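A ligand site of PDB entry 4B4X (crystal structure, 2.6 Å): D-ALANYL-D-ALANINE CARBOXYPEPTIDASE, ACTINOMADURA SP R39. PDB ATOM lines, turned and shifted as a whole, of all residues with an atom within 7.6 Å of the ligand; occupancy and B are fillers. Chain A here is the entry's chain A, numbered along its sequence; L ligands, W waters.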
ATOM      1  N   PRO A  47      11.853  -0.374 -13.302  1.00  0.00           N
ATOM      2  CA  PRO A  47      12.080   0.711 -12.331  1.00  0.00           C
ATOM      3  C   PRO A  47      13.059   0.377 -11.245  1.00  0.00           C
ATOM      4  O   PRO A  47      13.611   1.269 -10.618  1.00  0.00           O
ATOM      5  CB  PRO A  47      10.695   0.883 -11.695  1.00  0.00           C
ATOM      6  CG  PRO A  47      10.039  -0.473 -11.832  1.00  0.00           C
ATOM      7  CD  PRO A  47      10.649  -1.165 -13.013  1.00  0.00           C
ATOM      8  N   ALA A  48      13.275  -0.913 -11.021  1.00  0.00           N
ATOM      9  CA  ALA A  48      13.891  -1.446  -9.796  1.00  0.00           C
ATOM     10  C   ALA A  48      13.183  -0.808  -8.588  1.00  0.00           C
ATOM     11  O   ALA A  48      11.935  -0.796  -8.551  1.00  0.00           O
ATOM     12  CB  ALA A  48      15.381  -1.198  -9.788  1.00  0.00           C
ATOM     13  N   SER A  49      13.920  -0.279  -7.622  1.00  0.00           N
ATOM     14  CA  SER A  49      13.303   0.150  -6.385  1.00  0.00           C
ATOM     15  C   SER A  49      12.486   1.414  -6.468  1.00  0.00           C
ATOM     16  O   SER A  49      11.953   1.862  -5.463  1.00  0.00           O
ATOM     17  CB  SER A  49      14.306   0.174  -5.247  1.00  0.00           C
ATOM     18  OG  SER A  49      14.535  -1.165  -4.840  1.00  0.00           O
ATOM     19  N   ASN A  50      12.328   1.974  -7.655  1.00  0.00           N
ATOM     20  CA  ASN A  50      11.369   3.051  -7.847  1.00  0.00           C
ATOM     21  C   ASN A  50       9.913   2.541  -7.861  1.00  0.00           C
ATOM     22  O   ASN A  50       8.982   3.331  -7.858  1.00  0.00           O
ATOM     23  CB  ASN A  50      11.693   3.826  -9.122  1.00  0.00           C
ATOM     24  CG  ASN A  50      12.767   4.865  -8.905  1.00  0.00           C
ATOM     25  OD1 ASN A  50      13.689   4.648  -8.092  1.00  0.00           O
ATOM     26  ND2 ASN A  50      12.658   6.016  -9.610  1.00  0.00           N
ATOM     27  N   MET A  51       9.728   1.224  -7.874  1.00  0.00           N
ATOM     28  CA  MET A  51       8.395   0.616  -7.707  1.00  0.00           C
ATOM     29  C   MET A  51       7.892   0.850  -6.262  1.00  0.00           C
ATOM     30  O   MET A  51       6.678   0.744  -5.956  1.00  0.00           O
ATOM     31  CB  MET A  51       8.450  -0.891  -8.029  1.00  0.00           C
ATOM     32  CG  MET A  51       7.063  -1.563  -8.292  1.00  0.00           C
ATOM     33  SD  MET A  51       6.012  -0.590  -9.424  1.00  0.00           S
ATOM     34  CE  MET A  51       6.453  -1.322 -10.979  1.00  0.00           C
ATOM     35  N   LYS A  52       8.845   1.147  -5.376  1.00  0.00           N
ATOM     36  CA  LYS A  52       8.530   1.422  -3.990  1.00  0.00           C
ATOM     37  C   LYS A  52       7.769   2.706  -3.836  1.00  0.00           C
ATOM     38  O   LYS A  52       6.961   2.815  -2.913  1.00  0.00           O
ATOM     39  CB  LYS A  52       9.788   1.415  -3.120  1.00  0.00           C
ATOM     40  CG  LYS A  52      10.286   0.007  -2.897  1.00  0.00           C
ATOM     41  CD  LYS A  52      11.088  -0.142  -1.641  1.00  0.00           C
ATOM     42  CE  LYS A  52      11.303  -1.620  -1.311  1.00  0.00           C
ATOM     43  NZ  LYS A  52      12.282  -2.360  -2.212  1.00  0.00           N
ATOM     44  N   ASP A 142      19.025 -15.582  -5.078  1.00  0.00           N
ATOM     45  CA  ASP A 142      18.795 -14.445  -4.180  1.00  0.00           C
ATOM     46  C   ASP A 142      18.284 -14.868  -2.775  1.00  0.00           C
ATOM     47  O   ASP A 142      18.396 -14.132  -1.806  1.00  0.00           O
ATOM     48  CB  ASP A 142      17.738 -13.520  -4.794  1.00  0.00           C
ATOM     49  CG  ASP A 142      18.318 -12.503  -5.750  1.00  0.00           C
ATOM     50  OD1 ASP A 142      19.564 -12.377  -5.823  1.00  0.00           O
ATOM     51  OD2 ASP A 142      17.510 -11.808  -6.421  1.00  0.00           O
ATOM     52  N   ALA A 146      18.778 -10.716   2.805  1.00  0.00           N
ATOM     53  CA  ALA A 146      17.753  -9.852   3.387  1.00  0.00           C
ATOM     54  C   ALA A 146      16.745  -9.291   2.424  1.00  0.00           C
ATOM     55  O   ALA A 146      15.590  -9.078   2.793  1.00  0.00           O
ATOM     56  CB  ALA A 146      18.394  -8.703   4.167  1.00  0.00           C
ATOM     57  N   TYR A 147      17.169  -9.021   1.201  1.00  0.00           N
ATOM     58  CA  TYR A 147      16.295  -8.399   0.219  1.00  0.00           C
ATOM     59  C   TYR A 147      15.374  -9.427  -0.429  1.00  0.00           C
ATOM     60  O   TYR A 147      14.345  -9.073  -0.989  1.00  0.00           O
ATOM     61  CB  TYR A 147      17.113  -7.585  -0.829  1.00  0.00           C
ATOM     62  CG  TYR A 147      18.242  -8.385  -1.447  1.00  0.00           C
ATOM     63  CD1 TYR A 147      19.514  -8.402  -0.854  1.00  0.00           C
ATOM     64  CD2 TYR A 147      18.035  -9.155  -2.596  1.00  0.00           C
ATOM     65  CE1 TYR A 147      20.549  -9.136  -1.398  1.00  0.00           C
ATOM     66  CE2 TYR A 147      19.046  -9.889  -3.145  1.00  0.00           C
ATOM     67  CZ  TYR A 147      20.306  -9.881  -2.540  1.00  0.00           C
ATOM     68  OH  TYR A 147      21.339 -10.620  -3.068  1.00  0.00           O
ATOM     69  N   SER A 148      15.744 -10.697  -0.325  1.00  0.00           N
ATOM     70  CA  SER A 148      14.933 -11.801  -0.862  1.00  0.00           C
ATOM     71  C   SER A 148      14.348 -12.656   0.262  1.00  0.00           C
ATOM     72  O   SER A 148      14.008 -13.828   0.048  1.00  0.00           O
ATOM     73  CB  SER A 148      15.787 -12.678  -1.785  1.00  0.00           C
ATOM     74  OG  SER A 148      15.072 -13.813  -2.247  1.00  0.00           O
ATOM     75  N   PHE A 297      15.958   3.016   3.599  1.00  0.00           N
ATOM     76  CA  PHE A 297      16.867   1.911   3.289  1.00  0.00           C
ATOM     77  C   PHE A 297      16.372   0.950   2.176  1.00  0.00           C
ATOM     78  O   PHE A 297      16.955  -0.107   1.936  1.00  0.00           O
ATOM     79  CB  PHE A 297      17.203   1.124   4.586  1.00  0.00           C
ATOM     80  CG  PHE A 297      17.883   1.965   5.655  1.00  0.00           C
ATOM     81  CD1 PHE A 297      19.140   2.547   5.431  1.00  0.00           C
ATOM     82  CD2 PHE A 297      17.249   2.171   6.891  1.00  0.00           C
ATOM     83  CE1 PHE A 297      19.763   3.321   6.413  1.00  0.00           C
ATOM     84  CE2 PHE A 297      17.856   2.946   7.889  1.00  0.00           C
ATOM     85  CZ  PHE A 297      19.123   3.516   7.657  1.00  0.00           C
ATOM     86  N   SER A 298      15.286   1.333   1.505  1.00  0.00           N
ATOM     87  CA  SER A 298      14.687   0.496   0.470  1.00  0.00           C
ATOM     88  C   SER A 298      14.402  -0.932   0.982  1.00  0.00           C
ATOM     89  O   SER A 298      14.976  -1.918   0.505  1.00  0.00           O
ATOM     90  CB  SER A 298      15.608   0.495  -0.774  1.00  0.00           C
ATOM     91  OG  SER A 298      14.944   0.106  -1.959  1.00  0.00           O
ATOM     92  N   ASN A 299      13.510  -1.066   1.972  1.00  0.00           N
ATOM     93  CA  ASN A 299      13.114  -2.417   2.423  1.00  0.00           C
ATOM     94  C   ASN A 299      12.150  -3.142   1.478  1.00  0.00           C
ATOM     95  O   ASN A 299      11.000  -2.692   1.272  1.00  0.00           O
ATOM     96  CB  ASN A 299      12.538  -2.451   3.849  1.00  0.00           C
ATOM     97  CG  ASN A 299      12.746  -3.813   4.498  1.00  0.00           C
ATOM     98  OD1 ASN A 299      13.554  -3.941   5.399  1.00  0.00           O
ATOM     99  ND2 ASN A 299      12.038  -4.840   4.028  1.00  0.00           N
ATOM    100  N   ASN A 300      12.603  -4.273   0.934  1.00  0.00           N
ATOM    101  CA  ASN A 300      11.758  -5.091   0.084  1.00  0.00           C
ATOM    102  C   ASN A 300      10.647  -5.752   0.873  1.00  0.00           C
ATOM    103  O   ASN A 300       9.459  -5.599   0.535  1.00  0.00           O
ATOM    104  CB  ASN A 300      12.551  -6.211  -0.596  1.00  0.00           C
ATOM    105  CG  ASN A 300      13.524  -5.716  -1.604  1.00  0.00           C
ATOM    106  OD1 ASN A 300      13.407  -4.596  -2.191  1.00  0.00           O
ATOM    107  ND2 ASN A 300      14.497  -6.551  -1.860  1.00  0.00           N
ATOM    108  N   ASP A 345       5.096  -6.909  -8.455  1.00  0.00           N
ATOM    109  CA  ASP A 345       5.361  -6.864  -7.006  1.00  0.00           C
ATOM    110  C   ASP A 345       5.406  -5.423  -6.443  1.00  0.00           C
ATOM    111  O   ASP A 345       5.263  -4.436  -7.182  1.00  0.00           O
ATOM    112  CB  ASP A 345       6.650  -7.632  -6.622  1.00  0.00           C
ATOM    113  CG  ASP A 345       7.925  -6.858  -6.959  1.00  0.00           C
ATOM    114  OD1 ASP A 345       7.796  -5.668  -7.416  1.00  0.00           O
ATOM    115  OD2 ASP A 345       9.040  -7.440  -6.771  1.00  0.00           O
ATOM    116  N   SER A 347       8.041  -4.292  -4.172  1.00  0.00           N
ATOM    117  CA  SER A 347       9.393  -3.750  -3.976  1.00  0.00           C
ATOM    118  C   SER A 347      10.114  -3.255  -5.223  1.00  0.00           C
ATOM    119  O   SER A 347      10.934  -2.357  -5.145  1.00  0.00           O
ATOM    120  CB  SER A 347      10.282  -4.785  -3.266  1.00  0.00           C
ATOM    121  OG  SER A 347      10.550  -5.910  -4.073  1.00  0.00           O
ATOM    122  N   GLY A 348       9.806  -3.863  -6.369  1.00  0.00           N
ATOM    123  CA  GLY A 348      10.529  -3.583  -7.593  1.00  0.00           C
ATOM    124  C   GLY A 348      11.621  -4.621  -7.758  1.00  0.00           C
ATOM    125  O   GLY A 348      12.487  -4.443  -8.610  1.00  0.00           O
ATOM    126  N   LEU A 349      11.585  -5.680  -6.932  1.00  0.00           N
ATOM    127  CA  LEU A 349      12.539  -6.785  -7.038  1.00  0.00           C
ATOM    128  C   LEU A 349      12.279  -7.598  -8.302  1.00  0.00           C
ATOM    129  O   LEU A 349      13.230  -8.047  -8.972  1.00  0.00           O
ATOM    130  CB  LEU A 349      12.476  -7.704  -5.827  1.00  0.00           C
ATOM    131  CG  LEU A 349      13.708  -8.407  -5.234  1.00  0.00           C
ATOM    132  CD1 LEU A 349      13.200  -9.345  -4.178  1.00  0.00           C
ATOM    133  CD2 LEU A 349      14.641  -9.162  -6.196  1.00  0.00           C
ATOM    134  N   SER A 350      10.989  -7.800  -8.619  1.00  0.00           N
ATOM    135  CA  SER A 350      10.601  -8.504  -9.839  1.00  0.00           C
ATOM    136  C   SER A 350      11.041  -7.736 -11.084  1.00  0.00           C
ATOM    137  O   SER A 350      10.854  -6.513 -11.202  1.00  0.00           O
ATOM    138  CB  SER A 350       9.074  -8.732  -9.872  1.00  0.00           C
ATOM    139  OG  SER A 350       8.601  -9.152 -11.145  1.00  0.00           O
ATOM    140  N   THR A 393      19.679   5.625   1.357  1.00  0.00           N
ATOM    141  CA  THR A 393      20.549   5.150   0.290  1.00  0.00           C
ATOM    142  C   THR A 393      21.299   6.304  -0.390  1.00  0.00           C
ATOM    143  O   THR A 393      22.204   6.061  -1.211  1.00  0.00           O
ATOM    144  CB  THR A 393      19.782   4.359  -0.747  1.00  0.00           C
ATOM    145  OG1 THR A 393      18.555   5.030  -1.017  1.00  0.00           O
ATOM    146  CG2 THR A 393      19.489   2.961  -0.214  1.00  0.00           C
ATOM    147  N   LYS A 410      14.235   9.059  -4.478  1.00  0.00           N
ATOM    148  CA  LYS A 410      14.324   7.645  -4.175  1.00  0.00           C
ATOM    149  C   LYS A 410      15.103   6.976  -5.313  1.00  0.00           C
ATOM    150  O   LYS A 410      14.991   7.363  -6.480  1.00  0.00           O
ATOM    151  CB  LYS A 410      12.907   7.028  -4.001  1.00  0.00           C
ATOM    152  CG  LYS A 410      12.855   5.506  -3.915  1.00  0.00           C
ATOM    153  CD  LYS A 410      13.023   5.030  -2.516  1.00  0.00           C
ATOM    154  CE  LYS A 410      13.021   3.496  -2.451  1.00  0.00           C
ATOM    155  NZ  LYS A 410      14.344   2.879  -2.718  1.00  0.00           N
ATOM    156  N   THR A 411      15.875   5.972  -4.927  1.00  0.00           N
ATOM    157  CA  THR A 411      16.782   5.261  -5.799  1.00  0.00           C
ATOM    158  C   THR A 411      16.225   3.923  -6.208  1.00  0.00           C
ATOM    159  O   THR A 411      15.447   3.339  -5.484  1.00  0.00           O
ATOM    160  CB  THR A 411      18.079   4.938  -5.073  1.00  0.00           C
ATOM    161  OG1 THR A 411      17.789   4.212  -3.875  1.00  0.00           O
ATOM    162  CG2 THR A 411      18.812   6.214  -4.728  1.00  0.00           C
ATOM    163  N   GLY A 412      16.629   3.452  -7.366  1.00  0.00           N
ATOM    164  CA  GLY A 412      16.246   2.129  -7.826  1.00  0.00           C
ATOM    165  C   GLY A 412      17.478   1.485  -8.412  1.00  0.00           C
ATOM    166  O   GLY A 412      18.135   2.079  -9.252  1.00  0.00           O
ATOM    167  N   THR A 413      17.752   0.266  -7.971  1.00  0.00           N
ATOM    168  CA  THR A 413      18.986  -0.402  -8.362  1.00  0.00           C
ATOM    169  C   THR A 413      18.996  -1.961  -8.358  1.00  0.00           C
ATOM    170  O   THR A 413      18.656  -2.615  -7.360  1.00  0.00           O
ATOM    171  CB  THR A 413      20.175   0.125  -7.534  1.00  0.00           C
ATOM    172  OG1 THR A 413      21.329  -0.684  -7.800  1.00  0.00           O
ATOM    173  CG2 THR A 413      19.874   0.101  -6.039  1.00  0.00           C
ATOM    174  N   MET A 414      19.389  -2.531  -9.488  1.00  0.00           N
ATOM    175  CA  MET A 414      19.710  -3.962  -9.598  1.00  0.00           C
ATOM    176  C   MET A 414      20.495  -4.152 -10.865  1.00  0.00           C
ATOM    177  O   MET A 414      20.703  -3.176 -11.596  1.00  0.00           O
ATOM    178  CB  MET A 414      18.465  -4.851  -9.599  1.00  0.00           C
ATOM    179  CG  MET A 414      17.286  -4.296 -10.372  1.00  0.00           C
ATOM    180  SD  MET A 414      15.756  -5.262 -10.250  1.00  0.00           S
ATOM    181  CE  MET A 414      15.077  -4.765 -11.835  1.00  0.00           C
ATOM    182  N   SER A 415      20.944  -5.381 -11.140  1.00  0.00           N
ATOM    183  CA  SER A 415      21.698  -5.680 -12.355  1.00  0.00           C
ATOM    184  C   SER A 415      21.117  -4.952 -13.529  1.00  0.00           C
ATOM    185  O   SER A 415      19.922  -5.093 -13.803  1.00  0.00           O
ATOM    186  CB  SER A 415      21.715  -7.181 -12.632  1.00  0.00           C
ATOM    187  OG  SER A 415      23.056  -7.648 -12.584  1.00  0.00           O
ATOM    188  N   VAL A 417      19.974  -2.151 -14.040  1.00  0.00           N
ATOM    189  CA  VAL A 417      18.886  -1.181 -13.773  1.00  0.00           C
ATOM    190  C   VAL A 417      19.276  -0.147 -12.710  1.00  0.00           C
ATOM    191  O   VAL A 417      19.652  -0.499 -11.585  1.00  0.00           O
ATOM    192  CB  VAL A 417      17.564  -1.842 -13.357  1.00  0.00           C
ATOM    193  CG1 VAL A 417      16.442  -0.787 -13.302  1.00  0.00           C
ATOM    194  CG2 VAL A 417      17.194  -2.991 -14.306  1.00  0.00           C
ATOM    195  N   ALA A 419      18.049   3.865 -11.125  1.00  0.00           N
ATOM    196  CA  ALA A 419      17.016   4.907 -11.126  1.00  0.00           C
ATOM    197  C   ALA A 419      17.017   5.957 -10.002  1.00  0.00           C
ATOM    198  O   ALA A 419      17.311   5.679  -8.825  1.00  0.00           O
ATOM    199  CB  ALA A 419      15.643   4.278 -11.238  1.00  0.00           C
HETATM  200  O1  LIG L   1      19.152  -5.209  -3.858  1.00  0.00           O
HETATM  201  S1  LIG L   1      17.850  -5.207  -4.578  1.00  0.00           S
HETATM  202  O2  LIG L   1      16.905  -6.088  -3.825  1.00  0.00           O
HETATM  203  C1  LIG L   1      18.130  -5.864  -6.081  1.00  0.00           C
HETATM  204  N1  LIG L   1      17.361  -3.766  -4.763  1.00  0.00           N
HETATM  205  C2  LIG L   1      15.992  -3.351  -4.526  1.00  0.00           C
HETATM  206  C3  LIG L   1      15.092  -4.108  -5.470  1.00  0.00           C
HETATM  207  B1  LIG L   1      15.839  -1.782  -4.797  1.00  0.00           B
HETATM  208  O3  LIG L   1      16.494  -1.433  -6.140  1.00  0.00           O
HETATM  209  O4  LIG L   1      16.562  -1.060  -3.642  1.00  0.00           O
HETATM  210  O   HOH W   1      17.690   1.471  -3.895  1.00  0.00           O
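Ala 48 touches the ligand (CB to O3, 3.8 Å).
Tyr 147 touches the ligand.
C of Gly 412 touches O3 of the ligand (3.8 Å).
Met 414 touches the ligand (CB to C1, 3.7 Å).
Hydrophobic or aromatic side chains that line the ligand: Ala 48, Tyr 147 and Met 414.
Within 4 Å of the ligand: Ala 48, Ser 49, Tyr 147, Ser 298, Asn 300, Gly 412, Thr 413 and Met 414.
OD1 of Asn 300 is in hydrogen-bond range of NZ of Lys 52.
OG of Ser 298 lies within hydrogen-bond range of NZ of Lys 410 (2.9 Å).
The side-chain amide nitrogen (ND2) of Asn 300 sits at hydrogen-bond distance from the backbone carbonyl oxygen (O) of Tyr 147 (2.7 Å).
The side-chain amide oxygen of Asn 50 is in hydrogen-bond range of the backbone NH of Gly 412 (3.3 Å).
The side-chain hydroxyl (OG) of Ser 298 sits at hydrogen-bond distance from the side-chain hydroxyl (OG) of Ser 49.
The backbone carbonyl oxygen (O) of Gly 412 is in hydrogen-bond range of the backbone NH (N) of Ala 419, at 2.6 Å.
N of Ser 49 sits close to O3 of the ligand.
ND2 of Asn 300 is in hydrogen-bond range of O2 of the ligand (3.1 Å).
The side-chain hydroxyl (OG) of Ser 49 is covalently linked to a boron (B1) of the ligand (1.4 Å).
O of Thr 413 sits at hydrogen-bond distance from O3 of the ligand, at 2.7 Å.
An oxygen (O4) of the ligand is in hydrogen-bond range of the side-chain hydroxyl of Ser 298, at 2.6 Å.
An oxygen (O3) of the ligand lies within hydrogen-bond range of the backbone NH of Thr 413, at 2.8 Å.
Water W1 bridges the side-chain hydroxyl (OG1) of Thr 411 (2.7 Å) and an oxygen (O4) of the ligand (2.8 Å).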
